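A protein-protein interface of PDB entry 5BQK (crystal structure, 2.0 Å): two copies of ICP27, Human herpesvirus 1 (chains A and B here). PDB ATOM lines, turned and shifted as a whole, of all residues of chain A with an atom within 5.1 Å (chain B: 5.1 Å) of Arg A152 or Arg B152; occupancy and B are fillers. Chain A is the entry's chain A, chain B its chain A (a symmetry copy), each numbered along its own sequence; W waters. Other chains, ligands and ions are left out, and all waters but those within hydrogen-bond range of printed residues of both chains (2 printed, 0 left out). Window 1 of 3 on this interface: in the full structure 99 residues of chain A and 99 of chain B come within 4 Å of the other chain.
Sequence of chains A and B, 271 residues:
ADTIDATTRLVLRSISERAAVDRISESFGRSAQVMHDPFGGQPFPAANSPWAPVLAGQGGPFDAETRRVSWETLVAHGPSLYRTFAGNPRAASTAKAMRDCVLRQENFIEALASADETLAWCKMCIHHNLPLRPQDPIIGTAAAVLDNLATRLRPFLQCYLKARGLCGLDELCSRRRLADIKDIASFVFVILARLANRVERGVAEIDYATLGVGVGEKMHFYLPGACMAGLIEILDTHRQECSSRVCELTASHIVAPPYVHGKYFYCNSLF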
ATOM      1  N   ARG A 104     -27.863  -4.586  23.489  1.00  0.00           N
ATOM      2  CA  ARG A 104     -26.466  -4.242  23.940  1.00  0.00           C
ATOM      3  C   ARG A 104     -26.360  -3.446  25.211  1.00  0.00           C
ATOM      4  O   ARG A 104     -25.249  -3.286  25.725  1.00  0.00           O
ATOM      5  CB  ARG A 104     -25.608  -3.546  22.881  1.00  0.00           C
ATOM      6  CG  ARG A 104     -25.278  -4.533  21.722  1.00  0.00           C
ATOM      7  CD  ARG A 104     -24.909  -3.756  20.326  1.00  0.00           C
ATOM      8  NE  ARG A 104     -24.591  -4.797  19.331  1.00  0.00           N
ATOM      9  CZ  ARG A 104     -23.538  -5.615  19.343  1.00  0.00           C
ATOM     10  NH1 ARG A 104     -22.531  -5.531  20.228  1.00  0.00           N
ATOM     11  NH2 ARG A 104     -23.478  -6.548  18.395  1.00  0.00           N
ATOM     12  N   GLN A 105     -27.485  -2.952  25.723  1.00  0.00           N
ATOM     13  CA  GLN A 105     -27.464  -2.272  27.014  1.00  0.00           C
ATOM     14  C   GLN A 105     -28.311  -2.889  28.154  1.00  0.00           C
ATOM     15  O   GLN A 105     -28.481  -2.249  29.210  1.00  0.00           O
ATOM     16  CB  GLN A 105     -27.884  -0.815  26.790  1.00  0.00           C
ATOM     17  CG  GLN A 105     -29.367  -0.625  26.204  1.00  0.00           C
ATOM     18  CD  GLN A 105     -30.460  -0.712  27.258  1.00  0.00           C
ATOM     19  OE1 GLN A 105     -30.544   0.130  28.182  1.00  0.00           O
ATOM     20  NE2 GLN A 105     -31.268  -1.734  27.169  1.00  0.00           N
ATOM     21  N   GLU A 106     -28.891  -4.047  27.888  1.00  0.00           N
ATOM     22  CA  GLU A 106     -29.814  -4.780  28.761  1.00  0.00           C
ATOM     23  C   GLU A 106     -29.063  -5.236  29.948  1.00  0.00           C
ATOM     24  O   GLU A 106     -27.865  -5.503  29.829  1.00  0.00           O
ATOM     25  CB  GLU A 106     -30.280  -6.049  28.049  1.00  0.00           C
ATOM     26  CG  GLU A 106     -31.645  -5.854  27.546  1.00  0.00           C
ATOM     27  CD  GLU A 106     -32.225  -7.022  26.855  1.00  0.00           C
ATOM     28  OE1 GLU A 106     -31.512  -8.002  26.494  1.00  0.00           O
ATOM     29  OE2 GLU A 106     -33.469  -6.980  26.672  1.00  0.00           O
ATOM     30  N   ASN A 107     -29.744  -5.284  31.083  1.00  0.00           N
ATOM     31  CA  ASN A 107     -29.131  -5.931  32.291  1.00  0.00           C
ATOM     32  C   ASN A 107     -28.981  -7.475  32.150  1.00  0.00           C
ATOM     33  O   ASN A 107     -29.459  -8.066  31.227  1.00  0.00           O
ATOM     34  CB  ASN A 107     -29.808  -5.435  33.640  1.00  0.00           C
ATOM     35  CG  ASN A 107     -31.220  -6.042  33.854  1.00  0.00           C
ATOM     36  OD1 ASN A 107     -31.521  -7.137  33.339  1.00  0.00           O
ATOM     37  ND2 ASN A 107     -32.105  -5.316  34.618  1.00  0.00           N
ATOM     38  N   PHE A 108     -28.258  -8.117  33.056  1.00  0.00           N
ATOM     39  CA  PHE A 108     -28.006  -9.550  32.948  1.00  0.00           C
ATOM     40  C   PHE A 108     -29.233 -10.422  32.801  1.00  0.00           C
ATOM     41  O   PHE A 108     -29.375 -11.271  31.847  1.00  0.00           O
ATOM     42  CB  PHE A 108     -27.084 -10.009  34.099  1.00  0.00           C
ATOM     43  CG  PHE A 108     -26.728 -11.472  34.025  1.00  0.00           C
ATOM     44  CD1 PHE A 108     -25.909 -11.934  32.992  1.00  0.00           C
ATOM     45  CD2 PHE A 108     -27.208 -12.370  34.969  1.00  0.00           C
ATOM     46  CE1 PHE A 108     -25.574 -13.284  32.869  1.00  0.00           C
ATOM     47  CE2 PHE A 108     -26.893 -13.764  34.881  1.00  0.00           C
ATOM     48  CZ  PHE A 108     -26.049 -14.232  33.849  1.00  0.00           C
ATOM     49  N   ALA A 111     -30.705  -9.969  29.503  1.00  0.00           N
ATOM     50  CA  ALA A 111     -29.850 -10.477  28.448  1.00  0.00           C
ATOM     51  C   ALA A 111     -30.055 -12.005  28.409  1.00  0.00           C
ATOM     52  O   ALA A 111     -30.183 -12.589  27.357  1.00  0.00           O
ATOM     53  CB  ALA A 111     -28.381 -10.095  28.780  1.00  0.00           C
ATOM     54  N   ASN A 148     -23.318  -8.932  24.782  1.00  0.00           N
ATOM     55  CA  ASN A 148     -23.744  -8.517  26.118  1.00  0.00           C
ATOM     56  C   ASN A 148     -23.342  -9.599  27.169  1.00  0.00           C
ATOM     57  O   ASN A 148     -22.759  -9.337  28.254  1.00  0.00           O
ATOM     58  CB  ASN A 148     -25.287  -8.236  26.166  1.00  0.00           C
ATOM     59  CG  ASN A 148     -25.646  -7.247  27.329  1.00  0.00           C
ATOM     60  OD1 ASN A 148     -24.747  -6.711  27.883  1.00  0.00           O
ATOM     61  ND2 ASN A 148     -26.923  -7.023  27.664  1.00  0.00           N
ATOM     62  N   LEU A 149     -23.616 -10.823  26.830  1.00  0.00           N
ATOM     63  CA  LEU A 149     -23.428 -11.914  27.859  1.00  0.00           C
ATOM     64  C   LEU A 149     -21.913 -12.152  28.071  1.00  0.00           C
ATOM     65  O   LEU A 149     -21.428 -12.339  29.223  1.00  0.00           O
ATOM     66  CB  LEU A 149     -24.216 -13.152  27.424  1.00  0.00           C
ATOM     67  CG  LEU A 149     -25.743 -13.189  27.602  1.00  0.00           C
ATOM     68  CD1 LEU A 149     -26.399 -14.489  27.009  1.00  0.00           C
ATOM     69  CD2 LEU A 149     -26.084 -13.091  29.007  1.00  0.00           C
ATOM     70  N   ALA A 150     -21.153 -12.002  27.000  1.00  0.00           N
ATOM     71  CA  ALA A 150     -19.633 -12.082  27.073  1.00  0.00           C
ATOM     72  C   ALA A 150     -19.093 -11.038  27.961  1.00  0.00           C
ATOM     73  O   ALA A 150     -18.237 -11.345  28.819  1.00  0.00           O
ATOM     74  CB  ALA A 150     -18.977 -11.997  25.675  1.00  0.00           C
ATOM     75  N   THR A 151     -19.601  -9.790  27.824  1.00  0.00           N
ATOM     76  CA  THR A 151     -19.069  -8.716  28.673  1.00  0.00           C
ATOM     77  C   THR A 151     -19.240  -9.109  30.144  1.00  0.00           C
ATOM     78  O   THR A 151     -18.281  -9.082  30.895  1.00  0.00           O
ATOM     79  CB  THR A 151     -19.687  -7.348  28.327  1.00  0.00           C
ATOM     80  OG1 THR A 151     -19.263  -7.054  26.976  1.00  0.00           O
ATOM     81  CG2 THR A 151     -19.246  -6.250  29.264  1.00  0.00           C
ATOM     82  N   ARG A 152     -20.449  -9.479  30.504  1.00  0.00           N
ATOM     83  CA  ARG A 152     -20.888  -9.649  31.860  1.00  0.00           C
ATOM     84  C   ARG A 152     -20.347 -10.921  32.448  1.00  0.00           C
ATOM     85  O   ARG A 152     -19.931 -10.911  33.591  1.00  0.00           O
ATOM     86  CB  ARG A 152     -22.455  -9.654  31.923  1.00  0.00           C
ATOM     87  CG  ARG A 152     -23.038  -8.223  31.830  1.00  0.00           C
ATOM     88  CD  ARG A 152     -24.438  -8.272  31.241  1.00  0.00           C
ATOM     89  NE  ARG A 152     -24.844  -6.979  30.675  1.00  0.00           N
ATOM     90  CZ  ARG A 152     -25.306  -5.938  31.384  1.00  0.00           C
ATOM     91  NH1 ARG A 152     -25.600  -4.806  30.743  1.00  0.00           N
ATOM     92  NH2 ARG A 152     -25.421  -6.000  32.719  1.00  0.00           N
ATOM     93  N   LEU A 153     -20.243 -11.972  31.636  1.00  0.00           N
ATOM     94  CA  LEU A 153     -19.809 -13.281  32.148  1.00  0.00           C
ATOM     95  C   LEU A 153     -18.344 -13.601  32.016  1.00  0.00           C
ATOM     96  O   LEU A 153     -17.861 -14.520  32.728  1.00  0.00           O
ATOM     97  CB  LEU A 153     -20.652 -14.424  31.576  1.00  0.00           C
ATOM     98  CG  LEU A 153     -22.128 -14.392  31.995  1.00  0.00           C
ATOM     99  CD1 LEU A 153     -22.915 -15.495  31.346  1.00  0.00           C
ATOM    100  CD2 LEU A 153     -22.199 -14.605  33.464  1.00  0.00           C
ATOM    101  N   ARG A 154     -17.597 -12.846  31.200  1.00  0.00           N
ATOM    102  CA  ARG A 154     -16.191 -13.209  30.961  1.00  0.00           C
ATOM    103  C   ARG A 154     -15.318 -13.573  32.203  1.00  0.00           C
ATOM    104  O   ARG A 154     -14.694 -14.607  32.207  1.00  0.00           O
ATOM    105  CB  ARG A 154     -15.452 -12.166  30.103  1.00  0.00           C
ATOM    106  CG  ARG A 154     -14.001 -12.574  29.826  1.00  0.00           C
ATOM    107  CD  ARG A 154     -13.261 -11.588  28.854  1.00  0.00           C
ATOM    108  NE  ARG A 154     -13.405 -11.971  27.446  1.00  0.00           N
ATOM    109  CZ  ARG A 154     -14.316 -11.430  26.662  1.00  0.00           C
ATOM    110  NH1 ARG A 154     -15.104 -10.481  27.149  1.00  0.00           N
ATOM    111  NH2 ARG A 154     -14.419 -11.792  25.411  1.00  0.00           N
ATOM    112  N   PRO A 155     -15.255 -12.735  33.242  1.00  0.00           N
ATOM    113  CA  PRO A 155     -14.285 -13.112  34.288  1.00  0.00           C
ATOM    114  C   PRO A 155     -14.702 -14.356  35.123  1.00  0.00           C
ATOM    115  O   PRO A 155     -13.844 -15.117  35.664  1.00  0.00           O
ATOM    116  CB  PRO A 155     -14.197 -11.855  35.172  1.00  0.00           C
ATOM    117  CG  PRO A 155     -15.564 -11.189  34.957  1.00  0.00           C
ATOM    118  CD  PRO A 155     -15.831 -11.399  33.465  1.00  0.00           C
ATOM    119  N   ILE A 254     -22.682 -10.514  39.891  1.00  0.00           N
ATOM    120  CA  ILE A 254     -23.485 -10.698  38.682  1.00  0.00           C
ATOM    121  C   ILE A 254     -24.977 -10.968  38.960  1.00  0.00           C
ATOM    122  O   ILE A 254     -25.884 -10.312  38.374  1.00  0.00           O
ATOM    123  CB  ILE A 254     -22.915 -11.805  37.776  1.00  0.00           C
ATOM    124  CG1 ILE A 254     -21.632 -11.292  37.138  1.00  0.00           C
ATOM    125  CG2 ILE A 254     -23.922 -12.167  36.638  1.00  0.00           C
ATOM    126  CD1 ILE A 254     -20.843 -12.365  36.476  1.00  0.00           C
ATOM    127  N   ARG B 104     -18.755  -3.665  34.190  1.00  0.00           N
ATOM    128  CA  ARG B 104     -19.357  -4.522  33.107  1.00  0.00           C
ATOM    129  C   ARG B 104     -20.848  -4.423  32.936  1.00  0.00           C
ATOM    130  O   ARG B 104     -21.375  -4.961  31.959  1.00  0.00           O
ATOM    131  CB  ARG B 104     -18.997  -6.008  33.197  1.00  0.00           C
ATOM    132  CG  ARG B 104     -17.484  -6.214  32.890  1.00  0.00           C
ATOM    133  CD  ARG B 104     -16.901  -7.607  33.530  1.00  0.00           C
ATOM    134  NE  ARG B 104     -15.481  -7.692  33.142  1.00  0.00           N
ATOM    135  CZ  ARG B 104     -15.000  -7.867  31.910  1.00  0.00           C
ATOM    136  NH1 ARG B 104     -15.765  -8.107  30.833  1.00  0.00           N
ATOM    137  NH2 ARG B 104     -13.679  -7.828  31.759  1.00  0.00           N
ATOM    138  N   GLN B 105     -21.528  -3.748  33.861  1.00  0.00           N
ATOM    139  CA  GLN B 105     -22.959  -3.515  33.691  1.00  0.00           C
ATOM    140  C   GLN B 105     -23.432  -2.044  33.601  1.00  0.00           C
ATOM    141  O   GLN B 105     -24.650  -1.784  33.649  1.00  0.00           O
ATOM    142  CB  GLN B 105     -23.693  -4.224  34.834  1.00  0.00           C
ATOM    143  CG  GLN B 105     -23.322  -3.695  36.303  1.00  0.00           C
ATOM    144  CD  GLN B 105     -24.056  -2.424  36.703  1.00  0.00           C
ATOM    145  OE1 GLN B 105     -25.302  -2.406  36.836  1.00  0.00           O
ATOM    146  NE2 GLN B 105     -23.322  -1.355  36.851  1.00  0.00           N
ATOM    147  N   GLU B 106     -22.480  -1.126  33.571  1.00  0.00           N
ATOM    148  CA  GLU B 106     -22.671   0.328  33.584  1.00  0.00           C
ATOM    149  C   GLU B 106     -23.323   0.720  32.318  1.00  0.00           C
ATOM    150  O   GLU B 106     -23.092   0.061  31.300  1.00  0.00           O
ATOM    151  CB  GLU B 106     -21.306   1.015  33.581  1.00  0.00           C
ATOM    152  CG  GLU B 106     -21.005   1.509  34.930  1.00  0.00           C
ATOM    153  CD  GLU B 106     -19.717   2.219  35.059  1.00  0.00           C
ATOM    154  OE1 GLU B 106     -18.837   2.167  34.152  1.00  0.00           O
ATOM    155  OE2 GLU B 106     -19.571   2.888  36.114  1.00  0.00           O
ATOM    156  N   ASN B 107     -24.155   1.748  32.387  1.00  0.00           N
ATOM    157  CA  ASN B 107     -24.698   2.350  31.124  1.00  0.00           C
ATOM    158  C   ASN B 107     -23.619   3.098  30.286  1.00  0.00           C
ATOM    159  O   ASN B 107     -22.518   3.285  30.714  1.00  0.00           O
ATOM    160  CB  ASN B 107     -26.040   3.161  31.380  1.00  0.00           C
ATOM    161  CG  ASN B 107     -25.787   4.518  32.089  1.00  0.00           C
ATOM    162  OD1 ASN B 107     -24.690   5.097  31.969  1.00  0.00           O
ATOM    163  ND2 ASN B 107     -26.816   5.031  32.846  1.00  0.00           N
ATOM    164  N   PHE B 108     -23.934   3.475  29.056  1.00  0.00           N
ATOM    165  CA  PHE B 108     -22.952   4.109  28.183  1.00  0.00           C
ATOM    166  C   PHE B 108     -22.257   5.326  28.753  1.00  0.00           C
ATOM    167  O   PHE B 108     -20.978   5.439  28.802  1.00  0.00           O
ATOM    168  CB  PHE B 108     -23.578   4.377  26.796  1.00  0.00           C
ATOM    169  CG  PHE B 108     -22.607   4.980  25.815  1.00  0.00           C
ATOM    170  CD1 PHE B 108     -21.534   4.218  25.344  1.00  0.00           C
ATOM    171  CD2 PHE B 108     -22.760   6.288  25.374  1.00  0.00           C
ATOM    172  CE1 PHE B 108     -20.596   4.744  24.453  1.00  0.00           C
ATOM    173  CE2 PHE B 108     -21.819   6.870  24.464  1.00  0.00           C
ATOM    174  CZ  PHE B 108     -20.745   6.095  23.970  1.00  0.00           C
ATOM    175  N   ALA B 111     -19.949   4.332  31.386  1.00  0.00           N
ATOM    176  CA  ALA B 111     -18.832   3.563  30.872  1.00  0.00           C
ATOM    177  C   ALA B 111     -17.832   4.576  30.280  1.00  0.00           C
ATOM    178  O   ALA B 111     -16.645   4.474  30.489  1.00  0.00           O
ATOM    179  CB  ALA B 111     -19.367   2.576  29.798  1.00  0.00           C
ATOM    180  N   ASN B 148     -17.130  -3.313  27.990  1.00  0.00           N
ATOM    181  CA  ASN B 148     -18.416  -2.620  28.015  1.00  0.00           C
ATOM    182  C   ASN B 148     -18.559  -1.706  26.758  1.00  0.00           C
ATOM    183  O   ASN B 148     -19.580  -1.684  26.021  1.00  0.00           O
ATOM    184  CB  ASN B 148     -18.592  -1.788  29.334  1.00  0.00           C
ATOM    185  CG  ASN B 148     -20.109  -1.562  29.663  1.00  0.00           C
ATOM    186  OD1 ASN B 148     -20.899  -2.169  29.023  1.00  0.00           O
ATOM    187  ND2 ASN B 148     -20.478  -0.721  30.638  1.00  0.00           N
ATOM    188  N   LEU B 149     -17.516  -0.979  26.486  1.00  0.00           N
ATOM    189  CA  LEU B 149     -17.631   0.064  25.398  1.00  0.00           C
ATOM    190  C   LEU B 149     -17.683  -0.645  24.023  1.00  0.00           C
ATOM    191  O   LEU B 149     -18.470  -0.262  23.111  1.00  0.00           O
ATOM    192  CB  LEU B 149     -16.492   1.075  25.554  1.00  0.00           C
ATOM    193  CG  LEU B 149     -16.568   2.150  26.652  1.00  0.00           C
ATOM    194  CD1 LEU B 149     -15.271   3.035  26.734  1.00  0.00           C
ATOM    195  CD2 LEU B 149     -17.710   3.013  26.427  1.00  0.00           C
ATOM    196  N   ALA B 150     -16.966  -1.751  23.919  1.00  0.00           N
ATOM    197  CA  ALA B 150     -17.011  -2.627  22.673  1.00  0.00           C
ATOM    198  C   ALA B 150     -18.372  -3.140  22.438  1.00  0.00           C
ATOM    199  O   ALA B 150     -18.864  -3.067  21.291  1.00  0.00           O
ATOM    200  CB  ALA B 150     -15.997  -3.793  22.743  1.00  0.00           C
ATOM    201  N   THR B 151     -19.040  -3.625  23.511  1.00  0.00           N
ATOM    202  CA  THR B 151     -20.389  -4.170  23.312  1.00  0.00           C
ATOM    203  C   THR B 151     -21.277  -3.091  22.684  1.00  0.00           C
ATOM    204  O   THR B 151     -21.901  -3.335  21.666  1.00  0.00           O
ATOM    205  CB  THR B 151     -20.969  -4.762  24.610  1.00  0.00           C
ATOM    206  OG1 THR B 151     -20.118  -5.882  24.947  1.00  0.00           O
ATOM    207  CG2 THR B 151     -22.400  -5.220  24.461  1.00  0.00           C
ATOM    208  N   ARG B 152     -21.293  -1.928  23.297  1.00  0.00           N
ATOM    209  CA  ARG B 152     -22.226  -0.870  23.032  1.00  0.00           C
ATOM    210  C   ARG B 152     -21.893  -0.164  21.748  1.00  0.00           C
ATOM    211  O   ARG B 152     -22.795   0.141  20.993  1.00  0.00           O
ATOM    212  CB  ARG B 152     -22.232   0.153  24.220  1.00  0.00           C
ATOM    213  CG  ARG B 152     -23.048  -0.371  25.425  1.00  0.00           C
ATOM    214  CD  ARG B 152     -22.525   0.245  26.712  1.00  0.00           C
ATOM    215  NE  ARG B 152     -22.893  -0.547  27.893  1.00  0.00           N
ATOM    216  CZ  ARG B 152     -24.087  -0.516  28.502  1.00  0.00           C
ATOM    217  NH1 ARG B 152     -24.297  -1.322  29.544  1.00  0.00           N
ATOM    218  NH2 ARG B 152     -25.080   0.264  28.048  1.00  0.00           N
ATOM    219  N   LEU B 153     -20.603  -0.016  21.452  1.00  0.00           N
ATOM    220  CA  LEU B 153     -20.184   0.741  20.262  1.00  0.00           C
ATOM    221  C   LEU B 153     -19.916  -0.061  19.016  1.00  0.00           C
ATOM    222  O   LEU B 153     -19.900   0.536  17.907  1.00  0.00           O
ATOM    223  CB  LEU B 153     -18.998   1.662  20.561  1.00  0.00           C
ATOM    224  CG  LEU B 153     -19.306   2.785  21.561  1.00  0.00           C
ATOM    225  CD1 LEU B 153     -18.087   3.609  21.866  1.00  0.00           C
ATOM    226  CD2 LEU B 153     -20.309   3.693  20.945  1.00  0.00           C
ATOM    227  N   ARG B 154     -19.779  -1.388  19.129  1.00  0.00           N
ATOM    228  CA  ARG B 154     -19.401  -2.180  17.948  1.00  0.00           C
ATOM    229  C   ARG B 154     -20.155  -1.893  16.612  1.00  0.00           C
ATOM    230  O   ARG B 154     -19.522  -1.674  15.608  1.00  0.00           O
ATOM    231  CB  ARG B 154     -19.412  -3.694  18.227  1.00  0.00           C
ATOM    232  CG  ARG B 154     -18.977  -4.508  17.004  1.00  0.00           C
ATOM    233  CD  ARG B 154     -18.864  -6.046  17.298  1.00  0.00           C
ATOM    234  NE  ARG B 154     -17.527  -6.435  17.757  1.00  0.00           N
ATOM    235  CZ  ARG B 154     -17.238  -6.573  19.035  1.00  0.00           C
ATOM    236  NH1 ARG B 154     -18.194  -6.394  19.936  1.00  0.00           N
ATOM    237  NH2 ARG B 154     -16.037  -6.923  19.413  1.00  0.00           N
ATOM    238  N   PRO B 155     -21.491  -1.907  16.586  1.00  0.00           N
ATOM    239  CA  PRO B 155     -22.089  -1.771  15.243  1.00  0.00           C
ATOM    240  C   PRO B 155     -21.941  -0.353  14.623  1.00  0.00           C
ATOM    241  O   PRO B 155     -21.901  -0.173  13.368  1.00  0.00           O
ATOM    242  CB  PRO B 155     -23.570  -2.126  15.467  1.00  0.00           C
ATOM    243  CG  PRO B 155     -23.789  -1.765  16.944  1.00  0.00           C
ATOM    244  CD  PRO B 155     -22.493  -2.221  17.618  1.00  0.00           C
ATOM    245  N   ILE B 254     -27.861   4.804  20.909  1.00  0.00           N
ATOM    246  CA  ILE B 254     -26.787   4.814  21.903  1.00  0.00           C
ATOM    247  C   ILE B 254     -26.795   6.054  22.818  1.00  0.00           C
ATOM    248  O   ILE B 254     -26.731   5.945  24.075  1.00  0.00           O
ATOM    249  CB  ILE B 254     -25.400   4.653  21.253  1.00  0.00           C
ATOM    250  CG1 ILE B 254     -25.261   3.220  20.760  1.00  0.00           C
ATOM    251  CG2 ILE B 254     -24.264   4.932  22.288  1.00  0.00           C
ATOM    252  CD1 ILE B 254     -24.091   3.025  19.864  1.00  0.00           C
HETATM  253  O   HOH W   1     -27.366  -0.033  30.212  1.00  0.00           O
HETATM  254  O   HOH W   2     -26.854  -3.296  33.513  1.00  0.00           O
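Of the 15 printed residues of chain B, 6 touch a printed residue of chain A. Printed residues of chain B that touch a printed residue of chain A: Arg B104, Gln B105, Asn B148, Thr B151, Arg B152 and Pro B155. Hydrophobic or aromatic side chains of chain B that line the printed part of chain A: Pro B155. Among the printed residues, 12 pairs touch across the chains.
Water W1 bridges O of Gln A105 (2.7 Å) and NH2 of Arg B152 (3.2 Å). Water W2 bridges the backbone carbonyl oxygen of Gln B105 (2.7 Å) and the guanidinium group of Arg A152 (3.2 Å).
Arg A104 touches Arg B152, and with the chains exchanged Arg A152 touches Arg B104. Gln A105 touches Arg B152, and with the chains exchanged Arg A152 touches Gln B105. Thr A151 touches its own counterpart, Thr B151. Arg B152 touches its own counterpart, Arg A152. Positions printed for both chains: 104, 105, 106, 107, 108, 111, 148, 149, 150, 151, 152, 153, 154, 155 and 254. Of the 12 pairs that touch across the chains among the printed residues, 12 have their exchanged pair printed and touching as well.
O of Thr A151 lies within hydrogen-bond range of NH1 of Arg B104. O of Thr B151 lies within hydrogen-bond range of NH1 of Arg A104 (2.7 Å). OG1 of Thr A151 lies within hydrogen-bond range of OG1 of Thr B151 (2.5 Å).
The guanidinium group (NH1) of Arg B152 is in hydrogen-bond range of the backbone carbonyl oxygen (O) of Glu B106 (2.5 Å). OD1 of Asn A148 sits at hydrogen-bond distance from NE of Arg A152, at 2.8 Å. The side-chain amide oxygen of Asn B148 is in hydrogen-bond range of the guanidinium group of Arg B152, at 2.8 Å. O of Glu A106 lies within hydrogen-bond range of NH1 of Arg A152, 2.5 Å away. The backbone carbonyl oxygen of Glu B106 sits at hydrogen-bond distance from the side-chain amide nitrogen of Asn B148 (2.8 Å). ND2 of Asn A148 lies within hydrogen-bond range of O of Glu A106 (2.8 Å).
Printed residues of chain B within 4 Å of Thr A151: Arg B104 (2.7 Å), Asn B148 (3.8 Å) and Thr B151 (2.5 Å). Of the printed residues of chain B, Pro A155 touches Arg B104. Of the printed residues of chain A, Thr B151 touches Arg A104 (2.7 Å), Asn A148 (3.8 Å) and Thr A151 (2.5 Å). Of the printed residues of chain A, Arg B152 touches Arg A104, Gln A105 and Arg A152. The nearest printed residue of chain B that does not touch Arg A152 is Glu B106 (5.5 Å).
Arg A104 touches Arg B152. Arg A104 touches Pro B155. CB of Gln A105 touches NH2 of Arg B152, 3.3 Å away. N of Asn A148 touches CG2 of Thr B151, at 3.8 Å. Thr A151 touches Asn B148. Arg B104 touches Arg A152 (O to CG, 3.7 Å). Arg A152 touches Gln B105 (NH2 to CB, 3.3 Å). Arg B152 touches Arg A152. Pro A155 touches Arg B104.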
